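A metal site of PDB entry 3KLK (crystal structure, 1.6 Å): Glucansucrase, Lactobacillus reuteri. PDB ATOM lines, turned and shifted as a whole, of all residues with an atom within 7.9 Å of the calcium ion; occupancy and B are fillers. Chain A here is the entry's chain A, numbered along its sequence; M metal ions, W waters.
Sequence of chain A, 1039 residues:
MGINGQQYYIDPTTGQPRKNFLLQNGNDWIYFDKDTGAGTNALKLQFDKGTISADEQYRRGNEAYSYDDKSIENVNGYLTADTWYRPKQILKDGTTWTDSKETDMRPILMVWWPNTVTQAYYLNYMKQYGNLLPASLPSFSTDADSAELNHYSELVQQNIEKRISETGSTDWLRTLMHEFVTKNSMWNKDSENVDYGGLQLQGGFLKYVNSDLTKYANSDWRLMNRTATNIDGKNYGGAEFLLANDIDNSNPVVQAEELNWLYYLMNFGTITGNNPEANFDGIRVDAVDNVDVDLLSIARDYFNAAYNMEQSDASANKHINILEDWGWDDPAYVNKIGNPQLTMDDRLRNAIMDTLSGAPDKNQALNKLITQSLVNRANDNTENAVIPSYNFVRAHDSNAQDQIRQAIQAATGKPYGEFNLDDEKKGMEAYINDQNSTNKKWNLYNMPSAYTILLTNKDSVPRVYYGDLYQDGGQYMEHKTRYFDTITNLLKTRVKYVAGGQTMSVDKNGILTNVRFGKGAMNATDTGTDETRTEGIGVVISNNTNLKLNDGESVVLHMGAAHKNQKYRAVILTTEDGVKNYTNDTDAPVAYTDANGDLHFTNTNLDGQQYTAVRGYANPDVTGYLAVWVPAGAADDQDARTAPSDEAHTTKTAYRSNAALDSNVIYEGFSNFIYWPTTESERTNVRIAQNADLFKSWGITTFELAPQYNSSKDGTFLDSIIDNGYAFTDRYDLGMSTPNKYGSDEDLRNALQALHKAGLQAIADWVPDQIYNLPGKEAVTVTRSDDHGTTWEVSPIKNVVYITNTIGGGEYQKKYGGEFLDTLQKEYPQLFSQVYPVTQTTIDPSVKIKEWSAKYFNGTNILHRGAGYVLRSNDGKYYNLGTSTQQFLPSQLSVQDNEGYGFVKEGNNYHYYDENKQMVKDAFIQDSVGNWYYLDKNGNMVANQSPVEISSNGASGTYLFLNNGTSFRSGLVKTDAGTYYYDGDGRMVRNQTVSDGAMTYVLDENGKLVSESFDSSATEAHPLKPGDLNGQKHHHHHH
Within 4 Å of the calcium ion: Glu 240, Asp 246, Asn 290 and Asp 769.
The nearest printed residue that does not touch the calcium ion is Val 291 (4.3 Å).
The calcium ion is bound by the backbone carbonyl oxygen (O) of Glu 240 (2.3 Å), the backbone carbonyl oxygen (O) of Asn 290 (2.3 Å), water W1 (2.3 Å), the side-chain carboxylate (OD1) of Asp 246 (2.3 Å), the side-chain carboxylate (OE2) of Glu 240 (2.4 Å), the side-chain carboxylate (OD1) of Asp 769 (2.4 Å) and the side-chain carboxylate (OD2) of Asp 246 (2.5 Å).
The calcium ion has seven donor atoms within binding distance.
The side-chain carboxylate of Glu 240 sits close to the side-chain amide nitrogen of Asn 858 (3.4 Å).
OE1 of Glu 240 is in hydrogen-bond range of N of Asn 225, at 2.9 Å.
The backbone carbonyl oxygen of Asp 787 lies within hydrogen-bond range of the backbone NH of Glu 240, at 3.1 Å.
ND2 of Asn 290 sits at hydrogen-bond distance from O of Ala 239 (2.7 Å).
The backbone NH (N) of Asn 858 lies within hydrogen-bond range of the backbone carbonyl oxygen (O) of Asp 246 (2.7 Å).
O of Asp 769 is in hydrogen-bond range of N of Ile 247.
The side-chain carboxylate of Asp 769 lies close to the side-chain amide oxygen of Gln 770 (2.6 Å).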
ATOM      1  N   LEU A 223     -23.757  -7.952   2.601  1.00  0.00           N
ATOM      2  CA  LEU A 223     -23.796  -7.992   4.056  1.00  0.00           C
ATOM      3  C   LEU A 223     -24.081  -9.410   4.483  1.00  0.00           C
ATOM      4  O   LEU A 223     -25.206  -9.913   4.268  1.00  0.00           O
ATOM      5  CB  LEU A 223     -24.884  -7.056   4.588  1.00  0.00           C
ATOM      6  CG  LEU A 223     -24.775  -5.594   4.122  1.00  0.00           C
ATOM      7  CD1 LEU A 223     -25.830  -4.767   4.813  1.00  0.00           C
ATOM      8  CD2 LEU A 223     -23.407  -5.013   4.393  1.00  0.00           C
ATOM      9  N   MET A 224     -23.081 -10.083   5.073  1.00  0.00           N
ATOM     10  CA  MET A 224     -23.209 -11.534   5.279  1.00  0.00           C
ATOM     11  C   MET A 224     -23.562 -11.917   6.731  1.00  0.00           C
ATOM     12  O   MET A 224     -23.129 -11.190   7.657  1.00  0.00           O
ATOM     13  CB  MET A 224     -21.921 -12.248   4.846  1.00  0.00           C
ATOM     14  CG  MET A 224     -21.576 -12.043   3.389  1.00  0.00           C
ATOM     15  SD  MET A 224     -19.993 -12.799   3.000  1.00  0.00           S
ATOM     16  CE  MET A 224     -18.877 -11.550   3.676  1.00  0.00           C
ATOM     17  N   ASN A 225     -24.281 -13.040   6.903  1.00  0.00           N
ATOM     18  CA  ASN A 225     -24.539 -13.639   8.209  1.00  0.00           C
ATOM     19  C   ASN A 225     -25.458 -12.754   9.023  1.00  0.00           C
ATOM     20  O   ASN A 225     -25.427 -12.836  10.258  1.00  0.00           O
ATOM     21  CB  ASN A 225     -23.238 -13.867   9.036  1.00  0.00           C
ATOM     22  CG  ASN A 225     -22.076 -14.386   8.179  1.00  0.00           C
ATOM     23  OD1 ASN A 225     -22.253 -15.335   7.429  1.00  0.00           O
ATOM     24  ND2 ASN A 225     -20.874 -13.790   8.331  1.00  0.00           N
ATOM     25  N   GLY A 238     -25.862 -16.639  11.773  1.00  0.00           N
ATOM     26  CA  GLY A 238     -25.909 -17.904  11.047  1.00  0.00           C
ATOM     27  C   GLY A 238     -24.986 -17.843   9.848  1.00  0.00           C
ATOM     28  O   GLY A 238     -24.586 -16.754   9.431  1.00  0.00           O
ATOM     29  N   ALA A 239     -24.662 -18.999   9.277  1.00  0.00           N
ATOM     30  CA  ALA A 239     -23.747 -19.025   8.158  1.00  0.00           C
ATOM     31  C   ALA A 239     -24.410 -18.510   6.872  1.00  0.00           C
ATOM     32  O   ALA A 239     -25.415 -19.075   6.375  1.00  0.00           O
ATOM     33  CB  ALA A 239     -23.221 -20.476   7.934  1.00  0.00           C
ATOM     34  N   GLU A 240     -23.798 -17.488   6.265  1.00  0.00           N
ATOM     35  CA  GLU A 240     -24.344 -16.967   5.056  1.00  0.00           C
ATOM     36  C   GLU A 240     -24.294 -18.002   3.945  1.00  0.00           C
ATOM     37  O   GLU A 240     -25.223 -18.069   3.114  1.00  0.00           O
ATOM     38  CB  GLU A 240     -23.593 -15.686   4.607  1.00  0.00           C
ATOM     39  CG  GLU A 240     -24.220 -15.057   3.352  1.00  0.00           C
ATOM     40  CD  GLU A 240     -25.648 -14.579   3.637  1.00  0.00           C
ATOM     41  OE1 GLU A 240     -25.828 -13.813   4.633  1.00  0.00           O
ATOM     42  OE2 GLU A 240     -26.568 -14.971   2.875  1.00  0.00           O
ATOM     43  N   PHE A 241     -23.212 -18.771   3.896  1.00  0.00           N
ATOM     44  CA  PHE A 241     -22.979 -19.676   2.776  1.00  0.00           C
ATOM     45  C   PHE A 241     -23.450 -21.082   3.111  1.00  0.00           C
ATOM     46  O   PHE A 241     -23.188 -21.606   4.216  1.00  0.00           O
ATOM     47  CB  PHE A 241     -21.503 -19.747   2.426  1.00  0.00           C
ATOM     48  CG  PHE A 241     -20.988 -18.465   1.822  1.00  0.00           C
ATOM     49  CD1 PHE A 241     -21.221 -18.165   0.474  1.00  0.00           C
ATOM     50  CD2 PHE A 241     -20.292 -17.562   2.594  1.00  0.00           C
ATOM     51  CE1 PHE A 241     -20.742 -16.994  -0.099  1.00  0.00           C
ATOM     52  CE2 PHE A 241     -19.770 -16.358   2.021  1.00  0.00           C
ATOM     53  CZ  PHE A 241     -19.995 -16.085   0.675  1.00  0.00           C
ATOM     54  N   LEU A 242     -24.151 -21.694   2.158  1.00  0.00           N
ATOM     55  CA  LEU A 242     -24.746 -23.021   2.406  1.00  0.00           C
ATOM     56  C   LEU A 242     -24.465 -23.925   1.174  1.00  0.00           C
ATOM     57  O   LEU A 242     -23.760 -24.958   1.293  1.00  0.00           O
ATOM     58  CB  LEU A 242     -26.259 -22.878   2.626  1.00  0.00           C
ATOM     59  CG  LEU A 242     -27.047 -24.176   2.760  1.00  0.00           C
ATOM     60  CD1 LEU A 242     -26.527 -24.960   3.989  1.00  0.00           C
ATOM     61  CD2 LEU A 242     -28.533 -23.830   2.908  1.00  0.00           C
ATOM     62  N   LEU A 243     -24.996 -23.500   0.018  1.00  0.00           N
ATOM     63  CA  LEU A 243     -24.964 -24.312  -1.227  1.00  0.00           C
ATOM     64  C   LEU A 243     -24.868 -23.447  -2.483  1.00  0.00           C
ATOM     65  O   LEU A 243     -25.501 -22.399  -2.576  1.00  0.00           O
ATOM     66  CB  LEU A 243     -26.294 -25.109  -1.328  1.00  0.00           C
ATOM     67  CG  LEU A 243     -26.305 -26.302  -0.366  1.00  0.00           C
ATOM     68  CD1 LEU A 243     -27.777 -26.792  -0.125  1.00  0.00           C
ATOM     69  CD2 LEU A 243     -25.467 -27.432  -0.915  1.00  0.00           C
ATOM     70  N   ASN A 245     -24.727 -21.151  -5.653  1.00  0.00           N
ATOM     71  CA  ASN A 245     -24.512 -19.719  -5.819  1.00  0.00           C
ATOM     72  C   ASN A 245     -25.344 -18.955  -4.803  1.00  0.00           C
ATOM     73  O   ASN A 245     -26.574 -18.910  -4.911  1.00  0.00           O
ATOM     74  CB  ASN A 245     -24.881 -19.268  -7.225  1.00  0.00           C
ATOM     75  CG  ASN A 245     -24.079 -19.999  -8.288  1.00  0.00           C
ATOM     76  OD1 ASN A 245     -22.874 -19.762  -8.459  1.00  0.00           O
ATOM     77  ND2 ASN A 245     -24.720 -20.947  -8.947  1.00  0.00           N
ATOM     78  N   ASP A 246     -24.662 -18.334  -3.844  1.00  0.00           N
ATOM     79  CA  ASP A 246     -25.387 -17.726  -2.704  1.00  0.00           C
ATOM     80  C   ASP A 246     -25.938 -16.361  -3.092  1.00  0.00           C
ATOM     81  O   ASP A 246     -25.172 -15.430  -3.400  1.00  0.00           O
ATOM     82  CB  ASP A 246     -24.481 -17.596  -1.478  1.00  0.00           C
ATOM     83  CG  ASP A 246     -25.320 -17.344  -0.215  1.00  0.00           C
ATOM     84  OD1 ASP A 246     -26.112 -18.275   0.108  1.00  0.00           O
ATOM     85  OD2 ASP A 246     -25.196 -16.255   0.393  1.00  0.00           O
ATOM     86  N   ILE A 247     -27.261 -16.243  -3.116  1.00  0.00           N
ATOM     87  CA  ILE A 247     -27.862 -14.962  -3.444  1.00  0.00           C
ATOM     88  C   ILE A 247     -27.613 -13.876  -2.389  1.00  0.00           C
ATOM     89  O   ILE A 247     -27.753 -14.124  -1.185  1.00  0.00           O
ATOM     90  CB  ILE A 247     -29.383 -15.112  -3.650  1.00  0.00           C
ATOM     91  CG1 ILE A 247     -29.671 -15.931  -4.904  1.00  0.00           C
ATOM     92  CG2 ILE A 247     -30.048 -13.731  -3.786  1.00  0.00           C
ATOM     93  CD1 ILE A 247     -31.192 -16.315  -5.083  1.00  0.00           C
ATOM     94  N   ASP A 248     -27.258 -12.676  -2.846  1.00  0.00           N
ATOM     95  CA  ASP A 248     -26.986 -11.588  -1.898  1.00  0.00           C
ATOM     96  C   ASP A 248     -28.314 -10.947  -1.526  1.00  0.00           C
ATOM     97  O   ASP A 248     -28.733  -9.975  -2.167  1.00  0.00           O
ATOM     98  CB  ASP A 248     -26.046 -10.519  -2.483  1.00  0.00           C
ATOM     99  CG  ASP A 248     -25.834  -9.366  -1.517  1.00  0.00           C
ATOM    100  OD1 ASP A 248     -26.263  -9.484  -0.364  1.00  0.00           O
ATOM    101  OD2 ASP A 248     -25.236  -8.353  -1.912  1.00  0.00           O
ATOM    102  N   ASN A 249     -28.963 -11.512  -0.501  1.00  0.00           N
ATOM    103  CA  ASN A 249     -30.292 -11.015  -0.080  1.00  0.00           C
ATOM    104  C   ASN A 249     -30.233  -9.735   0.741  1.00  0.00           C
ATOM    105  O   ASN A 249     -31.270  -9.271   1.247  1.00  0.00           O
ATOM    106  CB  ASN A 249     -31.075 -12.108   0.642  1.00  0.00           C
ATOM    107  CG  ASN A 249     -31.511 -13.197  -0.312  1.00  0.00           C
ATOM    108  OD1 ASN A 249     -31.030 -14.385  -0.275  1.00  0.00           O
ATOM    109  ND2 ASN A 249     -32.357 -12.805  -1.230  1.00  0.00           N
ATOM    110  N   ALA A 287     -34.179 -22.248   4.777  1.00  0.00           N
ATOM    111  CA  ALA A 287     -32.806 -21.811   5.077  1.00  0.00           C
ATOM    112  C   ALA A 287     -32.809 -20.431   5.743  1.00  0.00           C
ATOM    113  O   ALA A 287     -31.982 -19.556   5.437  1.00  0.00           O
ATOM    114  CB  ALA A 287     -31.909 -21.828   3.790  1.00  0.00           C
ATOM    115  N   VAL A 288     -33.695 -20.277   6.738  1.00  0.00           N
ATOM    116  CA  VAL A 288     -33.817 -18.953   7.366  1.00  0.00           C
ATOM    117  C   VAL A 288     -32.445 -18.464   7.872  1.00  0.00           C
ATOM    118  O   VAL A 288     -32.072 -17.290   7.696  1.00  0.00           O
ATOM    119  CB  VAL A 288     -34.832 -18.990   8.513  1.00  0.00           C
ATOM    120  CG1 VAL A 288     -34.782 -17.678   9.293  1.00  0.00           C
ATOM    121  CG2 VAL A 288     -36.259 -19.198   7.928  1.00  0.00           C
ATOM    122  N   ASP A 289     -31.715 -19.333   8.542  1.00  0.00           N
ATOM    123  CA  ASP A 289     -30.491 -18.869   9.230  1.00  0.00           C
ATOM    124  C   ASP A 289     -29.274 -18.761   8.271  1.00  0.00           C
ATOM    125  O   ASP A 289     -28.123 -18.694   8.721  1.00  0.00           O
ATOM    126  CB  ASP A 289     -30.169 -19.769  10.414  1.00  0.00           C
ATOM    127  CG  ASP A 289     -31.192 -19.625  11.531  1.00  0.00           C
ATOM    128  OD1 ASP A 289     -31.875 -18.540  11.612  1.00  0.00           O
ATOM    129  OD2 ASP A 289     -31.279 -20.591  12.306  1.00  0.00           O
ATOM    130  N   ASN A 290     -29.545 -18.755   6.962  1.00  0.00           N
ATOM    131  CA  ASN A 290     -28.465 -18.555   5.954  1.00  0.00           C
ATOM    132  C   ASN A 290     -28.756 -17.399   5.047  1.00  0.00           C
ATOM    133  O   ASN A 290     -28.124 -17.244   3.981  1.00  0.00           O
ATOM    134  CB  ASN A 290     -28.352 -19.782   5.079  1.00  0.00           C
ATOM    135  CG  ASN A 290     -28.268 -21.029   5.888  1.00  0.00           C
ATOM    136  OD1 ASN A 290     -29.232 -21.820   5.959  1.00  0.00           O
ATOM    137  ND2 ASN A 290     -27.134 -21.200   6.546  1.00  0.00           N
ATOM    138  N   VAL A 291     -29.729 -16.577   5.449  1.00  0.00           N
ATOM    139  CA  VAL A 291     -30.056 -15.396   4.668  1.00  0.00           C
ATOM    140  C   VAL A 291     -30.262 -14.150   5.532  1.00  0.00           C
ATOM    141  O   VAL A 291     -30.482 -14.238   6.722  1.00  0.00           O
ATOM    142  CB  VAL A 291     -31.322 -15.603   3.770  1.00  0.00           C
ATOM    143  CG1 VAL A 291     -31.166 -16.819   2.884  1.00  0.00           C
ATOM    144  CG2 VAL A 291     -32.625 -15.723   4.658  1.00  0.00           C
ATOM    145  N   ASP A 292     -30.205 -12.990   4.877  1.00  0.00           N
ATOM    146  CA  ASP A 292     -30.462 -11.723   5.546  1.00  0.00           C
ATOM    147  C   ASP A 292     -31.900 -11.771   6.108  1.00  0.00           C
ATOM    148  O   ASP A 292     -32.870 -11.999   5.358  1.00  0.00           O
ATOM    149  CB  ASP A 292     -30.325 -10.588   4.498  1.00  0.00           C
ATOM    150  CG  ASP A 292     -30.787  -9.237   5.031  1.00  0.00           C
ATOM    151  OD1 ASP A 292     -31.158  -9.139   6.221  1.00  0.00           O
ATOM    152  OD2 ASP A 292     -30.745  -8.248   4.257  1.00  0.00           O
ATOM    153  N   PRO A 768     -35.121 -18.490  -1.150  1.00  0.00           N
ATOM    154  CA  PRO A 768     -34.285 -17.361  -1.583  1.00  0.00           C
ATOM    155  C   PRO A 768     -32.786 -17.547  -1.357  1.00  0.00           C
ATOM    156  O   PRO A 768     -32.006 -16.659  -1.734  1.00  0.00           O
ATOM    157  CB  PRO A 768     -34.818 -16.207  -0.751  1.00  0.00           C
ATOM    158  CG  PRO A 768     -35.241 -16.903   0.568  1.00  0.00           C
ATOM    159  CD  PRO A 768     -35.896 -18.186   0.066  1.00  0.00           C
ATOM    160  N   ASP A 769     -32.334 -18.657  -0.752  1.00  0.00           N
ATOM    161  CA  ASP A 769     -30.889 -18.677  -0.422  1.00  0.00           C
ATOM    162  C   ASP A 769     -29.925 -18.753  -1.634  1.00  0.00           C
ATOM    163  O   ASP A 769     -28.830 -18.171  -1.619  1.00  0.00           O
ATOM    164  CB  ASP A 769     -30.533 -19.845   0.478  1.00  0.00           C
ATOM    165  CG  ASP A 769     -29.038 -19.810   0.881  1.00  0.00           C
ATOM    166  OD1 ASP A 769     -28.646 -18.870   1.587  1.00  0.00           O
ATOM    167  OD2 ASP A 769     -28.288 -20.730   0.490  1.00  0.00           O
ATOM    168  N   GLN A 770     -30.292 -19.553  -2.629  1.00  0.00           N
ATOM    169  CA  GLN A 770     -29.332 -19.887  -3.692  1.00  0.00           C
ATOM    170  C   GLN A 770     -29.961 -20.318  -4.995  1.00  0.00           C
ATOM    171  O   GLN A 770     -31.163 -20.580  -5.070  1.00  0.00           O
ATOM    172  CB  GLN A 770     -28.311 -20.971  -3.206  1.00  0.00           C
ATOM    173  CG  GLN A 770     -28.890 -22.417  -3.244  1.00  0.00           C
ATOM    174  CD  GLN A 770     -29.856 -22.762  -2.060  1.00  0.00           C
ATOM    175  OE1 GLN A 770     -29.542 -22.519  -0.890  1.00  0.00           O
ATOM    176  NE2 GLN A 770     -31.002 -23.409  -2.395  1.00  0.00           N
ATOM    177  N   ASP A 787     -17.892 -20.784   5.984  1.00  0.00           N
ATOM    178  CA  ASP A 787     -19.320 -20.596   5.702  1.00  0.00           C
ATOM    179  C   ASP A 787     -19.858 -19.254   6.187  1.00  0.00           C
ATOM    180  O   ASP A 787     -21.032 -18.921   5.933  1.00  0.00           O
ATOM    181  CB  ASP A 787     -20.179 -21.776   6.272  1.00  0.00           C
ATOM    182  CG  ASP A 787     -20.090 -21.909   7.816  1.00  0.00           C
ATOM    183  OD1 ASP A 787     -19.539 -21.006   8.495  1.00  0.00           O
ATOM    184  OD2 ASP A 787     -20.626 -22.920   8.368  1.00  0.00           O
ATOM    185  N   ASN A 858     -23.234 -13.493  -3.238  1.00  0.00           N
ATOM    186  CA  ASN A 858     -22.232 -13.314  -2.164  1.00  0.00           C
ATOM    187  C   ASN A 858     -20.998 -14.155  -2.467  1.00  0.00           C
ATOM    188  O   ASN A 858     -19.894 -13.836  -1.993  1.00  0.00           O
ATOM    189  CB  ASN A 858     -22.792 -13.797  -0.840  1.00  0.00           C
ATOM    190  CG  ASN A 858     -23.769 -12.806  -0.232  1.00  0.00           C
ATOM    191  OD1 ASN A 858     -23.589 -11.610  -0.379  1.00  0.00           O
ATOM    192  ND2 ASN A 858     -24.794 -13.298   0.496  1.00  0.00           N
HETATM  193 CA    CA M   1     -27.003 -17.144   1.956  1.00  0.00          CA
HETATM  194  O   HOH W   1     -28.411 -16.136   0.380  1.00  0.00           O
